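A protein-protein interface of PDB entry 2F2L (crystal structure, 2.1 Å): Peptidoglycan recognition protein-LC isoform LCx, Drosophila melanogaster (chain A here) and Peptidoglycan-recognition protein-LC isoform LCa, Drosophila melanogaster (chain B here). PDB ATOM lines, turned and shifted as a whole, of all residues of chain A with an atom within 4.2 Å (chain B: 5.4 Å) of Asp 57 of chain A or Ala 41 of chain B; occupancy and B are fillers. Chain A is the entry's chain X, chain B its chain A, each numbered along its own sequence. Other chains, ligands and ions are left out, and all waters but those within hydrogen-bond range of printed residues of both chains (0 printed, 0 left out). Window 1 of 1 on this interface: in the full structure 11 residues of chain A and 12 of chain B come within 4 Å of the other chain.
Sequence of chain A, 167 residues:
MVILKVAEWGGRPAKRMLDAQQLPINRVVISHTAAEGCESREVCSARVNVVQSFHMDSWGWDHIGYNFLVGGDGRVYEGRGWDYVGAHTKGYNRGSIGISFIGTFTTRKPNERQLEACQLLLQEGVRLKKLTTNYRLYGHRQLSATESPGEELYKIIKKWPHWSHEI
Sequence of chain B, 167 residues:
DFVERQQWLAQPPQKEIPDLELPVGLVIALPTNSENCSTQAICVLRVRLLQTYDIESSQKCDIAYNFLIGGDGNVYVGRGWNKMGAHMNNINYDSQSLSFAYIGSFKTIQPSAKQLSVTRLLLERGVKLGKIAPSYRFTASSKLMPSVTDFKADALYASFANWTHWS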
ATOM      1  N   ARG A  12      24.972   6.428 -27.628  1.00  0.00           N
ATOM      2  CA  ARG A  12      26.353   5.939 -27.665  1.00  0.00           C
ATOM      3  C   ARG A  12      26.606   5.029 -28.843  1.00  0.00           C
ATOM      4  O   ARG A  12      25.688   4.377 -29.318  1.00  0.00           O
ATOM      5  CB  ARG A  12      26.624   5.085 -26.442  1.00  0.00           C
ATOM      6  CG  ARG A  12      26.552   5.798 -25.152  1.00  0.00           C
ATOM      7  CD  ARG A  12      26.940   4.824 -24.055  1.00  0.00           C
ATOM      8  NE  ARG A  12      25.779   4.408 -23.306  1.00  0.00           N
ATOM      9  CZ  ARG A  12      25.748   3.402 -22.442  1.00  0.00           C
ATOM     10  NH1 ARG A  12      26.810   2.628 -22.234  1.00  0.00           N
ATOM     11  NH2 ARG A  12      24.614   3.157 -21.811  1.00  0.00           N
ATOM     12  N   SER A  53      20.579   2.346 -22.444  1.00  0.00           N
ATOM     13  CA  SER A  53      21.196   2.058 -21.154  1.00  0.00           C
ATOM     14  C   SER A  53      20.753   0.706 -20.584  1.00  0.00           C
ATOM     15  O   SER A  53      21.552  -0.077 -20.081  1.00  0.00           O
ATOM     16  CB  SER A  53      20.849   3.173 -20.173  1.00  0.00           C
ATOM     17  OG  SER A  53      21.577   2.970 -18.979  1.00  0.00           O
ATOM     18  N   HIS A  55      19.743  -1.887 -22.292  1.00  0.00           N
ATOM     19  CA  HIS A  55      20.334  -2.943 -23.105  1.00  0.00           C
ATOM     20  C   HIS A  55      21.849  -3.054 -22.908  1.00  0.00           C
ATOM     21  O   HIS A  55      22.371  -4.155 -22.741  1.00  0.00           O
ATOM     22  CB  HIS A  55      19.953  -2.725 -24.569  1.00  0.00           C
ATOM     23  CG  HIS A  55      18.507  -2.984 -24.840  1.00  0.00           C
ATOM     24  ND1 HIS A  55      17.947  -2.848 -26.090  1.00  0.00           N
ATOM     25  CD2 HIS A  55      17.509  -3.406 -24.021  1.00  0.00           C
ATOM     26  CE1 HIS A  55      16.664  -3.160 -26.028  1.00  0.00           C
ATOM     27  NE2 HIS A  55      16.372  -3.505 -24.786  1.00  0.00           N
ATOM     28  N   MET A  56      22.535  -1.918 -22.858  1.00  0.00           N
ATOM     29  CA  MET A  56      24.008  -1.918 -22.772  1.00  0.00           C
ATOM     30  C   MET A  56      24.550  -2.062 -21.342  1.00  0.00           C
ATOM     31  O   MET A  56      25.592  -2.673 -21.142  1.00  0.00           O
ATOM     32  CB  MET A  56      24.606  -0.661 -23.425  1.00  0.00           C
ATOM     33  CG  MET A  56      24.409  -0.590 -24.945  1.00  0.00           C
ATOM     34  SD  MET A  56      25.015   0.923 -25.731  1.00  0.00           S
ATOM     35  CE  MET A  56      26.785   0.628 -25.722  1.00  0.00           C
ATOM     36  N   ASP A  57      23.859  -1.475 -20.371  1.00  0.00           N
ATOM     37  CA  ASP A  57      24.336  -1.433 -18.985  1.00  0.00           C
ATOM     38  C   ASP A  57      23.665  -2.499 -18.129  1.00  0.00           C
ATOM     39  O   ASP A  57      24.345  -3.242 -17.432  1.00  0.00           O
ATOM     40  CB  ASP A  57      24.144  -0.036 -18.372  1.00  0.00           C
ATOM     41  CG  ASP A  57      24.773   1.067 -19.216  1.00  0.00           C
ATOM     42  OD1 ASP A  57      25.813   0.811 -19.857  1.00  0.00           O
ATOM     43  OD2 ASP A  57      24.248   2.202 -19.235  1.00  0.00           O
ATOM     44  N   SER A  58      22.340  -2.578 -18.171  1.00  0.00           N
ATOM     45  CA  SER A  58      21.622  -3.530 -17.331  1.00  0.00           C
ATOM     46  C   SER A  58      21.724  -4.975 -17.862  1.00  0.00           C
ATOM     47  O   SER A  58      21.947  -5.898 -17.093  1.00  0.00           O
ATOM     48  CB  SER A  58      20.165  -3.096 -17.149  1.00  0.00           C
ATOM     49  OG  SER A  58      20.067  -1.769 -16.647  1.00  0.00           O
ATOM     50  N   TRP A  59      21.573  -5.182 -19.167  1.00  0.00           N
ATOM     51  CA  TRP A  59      21.782  -6.514 -19.755  1.00  0.00           C
ATOM     52  C   TRP A  59      23.216  -6.767 -20.180  1.00  0.00           C
ATOM     53  O   TRP A  59      23.619  -7.916 -20.340  1.00  0.00           O
ATOM     54  CB  TRP A  59      20.877  -6.731 -20.972  1.00  0.00           C
ATOM     55  CG  TRP A  59      19.421  -7.040 -20.640  1.00  0.00           C
ATOM     56  CD1 TRP A  59      18.333  -6.328 -21.027  1.00  0.00           C
ATOM     57  CD2 TRP A  59      18.928  -8.149 -19.886  1.00  0.00           C
ATOM     58  NE1 TRP A  59      17.180  -6.919 -20.556  1.00  0.00           N
ATOM     59  CE2 TRP A  59      17.521  -8.037 -19.845  1.00  0.00           C
ATOM     60  CE3 TRP A  59      19.538  -9.228 -19.232  1.00  0.00           C
ATOM     61  CZ2 TRP A  59      16.713  -8.971 -19.191  1.00  0.00           C
ATOM     62  CZ3 TRP A  59      18.743 -10.142 -18.580  1.00  0.00           C
ATOM     63  CH2 TRP A  59      17.341 -10.004 -18.551  1.00  0.00           C
ATOM     64  N   GLY A  60      23.975  -5.702 -20.409  1.00  0.00           N
ATOM     65  CA  GLY A  60      25.363  -5.834 -20.812  1.00  0.00           C
ATOM     66  C   GLY A  60      25.550  -6.154 -22.284  1.00  0.00           C
ATOM     67  O   GLY A  60      26.552  -6.753 -22.649  1.00  0.00           O
ATOM     68  N   THR B  39      24.682  -2.031  -8.136  1.00  0.00           N
ATOM     69  CA  THR B  39      24.866  -0.865  -8.982  1.00  0.00           C
ATOM     70  C   THR B  39      23.513  -0.462  -9.550  1.00  0.00           C
ATOM     71  O   THR B  39      22.623  -1.290  -9.653  1.00  0.00           O
ATOM     72  CB  THR B  39      25.849  -1.149 -10.142  1.00  0.00           C
ATOM     73  OG1 THR B  39      25.330  -2.195 -10.982  1.00  0.00           O
ATOM     74  CG2 THR B  39      27.214  -1.564  -9.598  1.00  0.00           C
ATOM     75  N   GLN B  40      23.364   0.809  -9.905  1.00  0.00           N
ATOM     76  CA  GLN B  40      22.111   1.307 -10.485  1.00  0.00           C
ATOM     77  C   GLN B  40      21.658   0.490 -11.700  1.00  0.00           C
ATOM     78  O   GLN B  40      20.491   0.171 -11.825  1.00  0.00           O
ATOM     79  CB  GLN B  40      22.221   2.790 -10.853  1.00  0.00           C
ATOM     80  CG  GLN B  40      20.922   3.375 -11.391  1.00  0.00           C
ATOM     81  CD  GLN B  40      20.909   4.888 -11.393  1.00  0.00           C
ATOM     82  OE1 GLN B  40      21.427   5.523 -10.486  1.00  0.00           O
ATOM     83  NE2 GLN B  40      20.292   5.472 -12.406  1.00  0.00           N
ATOM     84  N   ALA B  41      22.585   0.133 -12.581  1.00  0.00           N
ATOM     85  CA  ALA B  41      22.226  -0.612 -13.791  1.00  0.00           C
ATOM     86  C   ALA B  41      21.585  -1.977 -13.485  1.00  0.00           C
ATOM     87  O   ALA B  41      20.627  -2.396 -14.153  1.00  0.00           O
ATOM     88  CB  ALA B  41      23.452  -0.787 -14.693  1.00  0.00           C
ATOM     89  N   ILE B  42      22.109  -2.673 -12.480  1.00  0.00           N
ATOM     90  CA  ILE B  42      21.554  -3.975 -12.117  1.00  0.00           C
ATOM     91  C   ILE B  42      20.271  -3.815 -11.305  1.00  0.00           C
ATOM     92  O   ILE B  42      19.333  -4.591 -11.470  1.00  0.00           O
ATOM     93  CB  ILE B  42      22.577  -4.844 -11.364  1.00  0.00           C
ATOM     94  CG1 ILE B  42      23.832  -5.077 -12.226  1.00  0.00           C
ATOM     95  CG2 ILE B  42      21.942  -6.164 -10.927  1.00  0.00           C
ATOM     96  CD1 ILE B  42      23.580  -5.621 -13.628  1.00  0.00           C
ATOM     97  N   CYS B  43      20.221  -2.814 -10.426  1.00  0.00           N
ATOM     98  CA  CYS B  43      18.987  -2.533  -9.684  1.00  0.00           C
ATOM     99  C   CYS B  43      17.840  -2.206 -10.626  1.00  0.00           C
ATOM    100  O   CYS B  43      16.725  -2.672 -10.421  1.00  0.00           O
ATOM    101  CB  CYS B  43      19.180  -1.399  -8.684  1.00  0.00           C
ATOM    102  SG  CYS B  43      20.246  -1.815  -7.257  1.00  0.00           S
ATOM    103  N   VAL B  44      18.116  -1.407 -11.650  1.00  0.00           N
ATOM    104  CA  VAL B  44      17.127  -1.100 -12.663  1.00  0.00           C
ATOM    105  C   VAL B  44      16.591  -2.389 -13.312  1.00  0.00           C
ATOM    106  O   VAL B  44      15.392  -2.521 -13.494  1.00  0.00           O
ATOM    107  CB  VAL B  44      17.676  -0.107 -13.731  1.00  0.00           C
ATOM    108  CG1 VAL B  44      16.882  -0.180 -15.047  1.00  0.00           C
ATOM    109  CG2 VAL B  44      17.656   1.331 -13.185  1.00  0.00           C
ATOM    110  N   LEU B  45      17.488  -3.317 -13.650  1.00  0.00           N
ATOM    111  CA  LEU B  45      17.103  -4.634 -14.168  1.00  0.00           C
ATOM    112  C   LEU B  45      16.189  -5.350 -13.192  1.00  0.00           C
ATOM    113  O   LEU B  45      15.132  -5.888 -13.571  1.00  0.00           O
ATOM    114  CB  LEU B  45      18.343  -5.500 -14.426  1.00  0.00           C
ATOM    115  CG  LEU B  45      18.111  -6.850 -15.113  1.00  0.00           C
ATOM    116  CD1 LEU B  45      17.458  -6.655 -16.471  1.00  0.00           C
ATOM    117  CD2 LEU B  45      19.424  -7.595 -15.257  1.00  0.00           C
ATOM    118  N   TYR B  76      14.173   3.483  -5.561  1.00  0.00           N
ATOM    119  CA  TYR B  76      13.501   3.314  -6.864  1.00  0.00           C
ATOM    120  C   TYR B  76      12.025   3.607  -6.661  1.00  0.00           C
ATOM    121  O   TYR B  76      11.386   3.023  -5.809  1.00  0.00           O
ATOM    122  CB  TYR B  76      13.764   1.900  -7.410  1.00  0.00           C
ATOM    123  CG  TYR B  76      15.213   1.781  -7.772  1.00  0.00           C
ATOM    124  CD1 TYR B  76      15.630   1.938  -9.072  1.00  0.00           C
ATOM    125  CD2 TYR B  76      16.183   1.614  -6.787  1.00  0.00           C
ATOM    126  CE1 TYR B  76      16.972   1.885  -9.408  1.00  0.00           C
ATOM    127  CE2 TYR B  76      17.533   1.567  -7.105  1.00  0.00           C
ATOM    128  CZ  TYR B  76      17.923   1.718  -8.420  1.00  0.00           C
ATOM    129  OH  TYR B  76      19.249   1.684  -8.769  1.00  0.00           O
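Printed residues of chain B within 4 Å of Asp 57 of chain A: Ala 41 (3.8 Å).
Ala 41 of chain B touches two residues of chain A.
Printed residues of chain B within 4 Å of Trp 59 of chain A: Leu 45.
Of the printed residues of chain A, Leu 45 of chain B touches Ser 58 and Trp 59.
Of the printed residues of chain B, Ser 58 of chain A touches Ala 41 (2.6 Å), Ile 42 (3.8 Å), Val 44 (3.9 Å) and Leu 45 (3.6 Å).
Met 56 of chain A touches none of the printed residues of chain B.
The nearest printed residue of chain A that does not touch Ala 41 of chain B is Ser 53 of chain A (5.8 Å).
The nearest printed residue of chain A that does not touch Ile 42 of chain B is Asp 57 of chain A (4.6 Å).
Printed residues of chain A that touch a printed residue of chain B: Asp 57, Ser 58 and Trp 59.
Hydrophobic or aromatic side chains of chain A that line the printed part of chain B: Trp 59.
Along chain A the printed residues that touch a printed residue of chain B span positions 57 to 59.
Printed residues of chain B that touch a printed residue of chain A: Ala 41, Ile 42, Val 44 and Leu 45.
Hydrophobic or aromatic side chains of chain B within 4 Å of the printed part of chain A: Ala 41, Ile 42, Val 44 and Leu 45.
Among the printed residues, 6 pairs touch across the chains.
Among the printed residues, no Asp or Glu carboxylate lies within 4 Å of a Lys or Arg side-chain nitrogen of the other chain.
The backbone NH (N) of Ser 58 of chain A lies within hydrogen-bond range of the backbone carbonyl oxygen (O) of Ser 53 of chain A (3.2 Å).
OD2 of Asp 57 of chain A is in salt-bridge range of NH2 of Arg 12 of chain A, at 2.8 Å.
OD2 of Asp 57 of chain A lies within hydrogen-bond range of OG of Ser 53 of chain A (2.8 Å).
Asp 57 of chain A touches Ala 41 of chain B.
Ile 42 of chain B touches Ser 58 of chain A.
Ser 58 of chain A touches Val 44 of chain B.
O of Ser 58 of chain A touches CD2 of Leu 45 of chain B, 3.6 Å away.
Leu 45 of chain B touches Trp 59 of chain A.
The backbone carbonyl oxygen of Ala 41 of chain B is in hydrogen-bond range of the side-chain hydroxyl of Ser 58 of chain A (2.6 Å).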
